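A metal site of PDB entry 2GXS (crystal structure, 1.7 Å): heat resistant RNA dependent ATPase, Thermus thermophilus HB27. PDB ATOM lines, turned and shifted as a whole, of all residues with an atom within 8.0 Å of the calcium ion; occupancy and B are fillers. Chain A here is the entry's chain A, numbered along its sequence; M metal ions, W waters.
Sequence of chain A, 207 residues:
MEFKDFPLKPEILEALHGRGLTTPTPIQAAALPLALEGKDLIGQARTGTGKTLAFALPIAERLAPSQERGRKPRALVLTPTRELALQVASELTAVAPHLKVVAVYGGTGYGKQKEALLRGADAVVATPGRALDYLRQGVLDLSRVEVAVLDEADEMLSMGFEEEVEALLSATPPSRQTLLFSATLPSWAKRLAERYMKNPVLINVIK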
ATOM      1  N   PRO A 128     -20.554  11.327  -2.924  1.00  0.00           N
ATOM      2  CA  PRO A 128     -20.770  11.098  -1.488  1.00  0.00           C
ATOM      3  C   PRO A 128     -19.525  10.602  -0.697  1.00  0.00           C
ATOM      4  O   PRO A 128     -19.354  10.948   0.474  1.00  0.00           O
ATOM      5  CB  PRO A 128     -21.908  10.083  -1.440  1.00  0.00           C
ATOM      6  CG  PRO A 128     -22.544  10.182  -2.759  1.00  0.00           C
ATOM      7  CD  PRO A 128     -21.433  10.471  -3.736  1.00  0.00           C
ATOM      8  N   GLY A 129     -18.683   9.844  -1.351  1.00  0.00           N
ATOM      9  CA  GLY A 129     -17.489   9.300  -0.690  1.00  0.00           C
ATOM     10  C   GLY A 129     -16.523  10.398  -0.305  1.00  0.00           C
ATOM     11  O   GLY A 129     -16.099  10.523   0.843  1.00  0.00           O
ATOM     12  N   LEU A 132     -17.852  12.736   2.290  1.00  0.00           N
ATOM     13  CA  LEU A 132     -17.873  12.249   3.673  1.00  0.00           C
ATOM     14  C   LEU A 132     -16.470  12.383   4.260  1.00  0.00           C
ATOM     15  O   LEU A 132     -16.328  12.691   5.441  1.00  0.00           O
ATOM     16  CB  LEU A 132     -18.398  10.810   3.789  1.00  0.00           C
ATOM     17  CG  LEU A 132     -18.544  10.227   5.203  1.00  0.00           C
ATOM     18  CD1 LEU A 132     -19.498  11.039   6.043  1.00  0.00           C
ATOM     19  CD2 LEU A 132     -19.029   8.734   5.150  1.00  0.00           C
ATOM     20  N   MET A 156     -26.847   6.428  -6.881  1.00  0.00           N
ATOM     21  CA  MET A 156     -26.039   6.514  -5.651  1.00  0.00           C
ATOM     22  C   MET A 156     -26.173   5.173  -4.870  1.00  0.00           C
ATOM     23  O   MET A 156     -25.206   4.617  -4.324  1.00  0.00           O
ATOM     24  CB  MET A 156     -26.450   7.738  -4.816  1.00  0.00           C
ATOM     25  CG  MET A 156     -25.958   9.015  -5.471  1.00  0.00           C
ATOM     26  SD  MET A 156     -25.889  10.496  -4.470  1.00  0.00           S
ATOM     27  CE  MET A 156     -27.607  10.728  -4.163  1.00  0.00           C
ATOM     28  N   LEU A 157     -27.400   4.648  -4.864  1.00  0.00           N
ATOM     29  CA  LEU A 157     -27.675   3.379  -4.222  1.00  0.00           C
ATOM     30  C   LEU A 157     -26.890   2.291  -4.923  1.00  0.00           C
ATOM     31  O   LEU A 157     -26.195   1.486  -4.296  1.00  0.00           O
ATOM     32  CB  LEU A 157     -29.157   3.071  -4.338  1.00  0.00           C
ATOM     33  CG  LEU A 157     -29.576   1.689  -3.811  1.00  0.00           C
ATOM     34  CD1 LEU A 157     -29.319   1.610  -2.320  1.00  0.00           C
ATOM     35  CD2 LEU A 157     -31.059   1.481  -4.189  1.00  0.00           C
ATOM     36  N   MET A 159     -24.272   2.241  -6.575  1.00  0.00           N
ATOM     37  CA  MET A 159     -22.816   2.355  -6.395  1.00  0.00           C
ATOM     38  C   MET A 159     -22.322   2.139  -4.990  1.00  0.00           C
ATOM     39  O   MET A 159     -21.106   2.149  -4.727  1.00  0.00           O
ATOM     40  CB  MET A 159     -22.385   3.754  -6.760  1.00  0.00           C
ATOM     41  CG  MET A 159     -22.542   4.010  -8.163  1.00  0.00           C
ATOM     42  SD  MET A 159     -22.340   5.737  -8.374  1.00  0.00           S
ATOM     43  CE  MET A 159     -21.207   5.749  -9.762  1.00  0.00           C
ATOM     44  N   GLY A 160     -23.244   1.971  -4.063  1.00  0.00           N
ATOM     45  CA  GLY A 160     -22.901   1.672  -2.697  1.00  0.00           C
ATOM     46  C   GLY A 160     -22.777   2.873  -1.801  1.00  0.00           C
ATOM     47  O   GLY A 160     -22.160   2.786  -0.749  1.00  0.00           O
ATOM     48  N   PHE A 161     -23.389   4.006  -2.175  1.00  0.00           N
ATOM     49  CA  PHE A 161     -23.263   5.247  -1.380  1.00  0.00           C
ATOM     50  C   PHE A 161     -24.351   5.472  -0.303  1.00  0.00           C
ATOM     51  O   PHE A 161     -24.489   6.556   0.277  1.00  0.00           O
ATOM     52  CB  PHE A 161     -23.198   6.468  -2.284  1.00  0.00           C
ATOM     53  CG  PHE A 161     -21.982   6.536  -3.150  1.00  0.00           C
ATOM     54  CD1 PHE A 161     -20.707   6.370  -2.598  1.00  0.00           C
ATOM     55  CD2 PHE A 161     -22.107   6.833  -4.484  1.00  0.00           C
ATOM     56  CE1 PHE A 161     -19.595   6.472  -3.400  1.00  0.00           C
ATOM     57  CE2 PHE A 161     -21.011   6.906  -5.301  1.00  0.00           C
ATOM     58  CZ  PHE A 161     -19.757   6.733  -4.760  1.00  0.00           C
ATOM     59  N   GLU A 162     -25.130   4.424  -0.005  1.00  0.00           N
ATOM     60  CA  GLU A 162     -26.250   4.586   0.898  1.00  0.00           C
ATOM     61  C   GLU A 162     -25.770   5.166   2.245  1.00  0.00           C
ATOM     62  O   GLU A 162     -26.361   6.106   2.766  1.00  0.00           O
ATOM     63  CB  GLU A 162     -27.070   3.276   0.999  1.00  0.00           C
ATOM     64  CG  GLU A 162     -26.247   1.971   1.196  1.00  0.00           C
ATOM     65  CD  GLU A 162     -27.090   0.723   1.081  1.00  0.00           C
ATOM     66  OE1 GLU A 162     -27.750   0.262   2.046  1.00  0.00           O
ATOM     67  OE2 GLU A 162     -27.092   0.190   0.022  1.00  0.00           O
ATOM     68  N   GLU A 163     -24.676   4.633   2.771  1.00  0.00           N
ATOM     69  CA  GLU A 163     -24.225   5.013   4.090  1.00  0.00           C
ATOM     70  C   GLU A 163     -23.714   6.434   4.109  1.00  0.00           C
ATOM     71  O   GLU A 163     -23.973   7.195   5.031  1.00  0.00           O
ATOM     72  CB  GLU A 163     -23.145   4.044   4.583  1.00  0.00           C
ATOM     73  CG  GLU A 163     -23.590   2.557   4.531  1.00  0.00           C
ATOM     74  CD  GLU A 163     -23.330   1.813   3.208  1.00  0.00           C
ATOM     75  OE1 GLU A 163     -22.912   2.432   2.217  1.00  0.00           O
ATOM     76  OE2 GLU A 163     -23.542   0.563   3.197  1.00  0.00           O
ATOM     77  N   GLU A 164     -22.984   6.786   3.052  1.00  0.00           N
ATOM     78  CA  GLU A 164     -22.345   8.107   2.964  1.00  0.00           C
ATOM     79  C   GLU A 164     -23.439   9.193   2.843  1.00  0.00           C
ATOM     80  O   GLU A 164     -23.419  10.248   3.495  1.00  0.00           O
ATOM     81  CB  GLU A 164     -21.436   8.160   1.754  1.00  0.00           C
ATOM     82  CG  GLU A 164     -20.144   7.275   1.839  1.00  0.00           C
ATOM     83  CD  GLU A 164     -20.349   5.766   1.603  1.00  0.00           C
ATOM     84  OE1 GLU A 164     -21.397   5.309   1.113  1.00  0.00           O
ATOM     85  OE2 GLU A 164     -19.426   4.990   1.945  1.00  0.00           O
ATOM     86  N   VAL A 165     -24.404   8.917   1.974  1.00  0.00           N
ATOM     87  CA  VAL A 165     -25.519   9.833   1.804  1.00  0.00           C
ATOM     88  C   VAL A 165     -26.319  10.055   3.077  1.00  0.00           C
ATOM     89  O   VAL A 165     -26.650  11.189   3.419  1.00  0.00           O
ATOM     90  CB  VAL A 165     -26.471   9.352   0.657  1.00  0.00           C
ATOM     91  CG1 VAL A 165     -27.781  10.130   0.708  1.00  0.00           C
ATOM     92  CG2 VAL A 165     -25.781   9.487  -0.705  1.00  0.00           C
HETATM   93 CA    CA M   1     -20.773   2.882   1.103  1.00  0.00          CA
HETATM   94  O   HOH W   1     -20.412   0.551   0.271  1.00  0.00           O
HETATM   95  O   HOH W   2     -19.118   3.189  -0.622  1.00  0.00           O
HETATM   96  O   HOH W   3     -18.886   1.605   2.249  1.00  0.00           O
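The nearest printed residue that does not touch the calcium ion is Phe 161 (4.2 Å).
The calcium ion is bound by the backbone carbonyl oxygen (O) of Gly 160 (2.3 Å), water W2 (2.4 Å), the side-chain carboxylate (OE1) of Glu 163 (2.5 Å), water W1 (2.5 Å), the side-chain carboxylate (OE1) of Glu 164 (2.5 Å), water W3 (2.6 Å) and the side-chain carboxylate (OE2) of Glu 164 (2.6 Å).
The calcium ion has seven donor atoms within binding distance.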
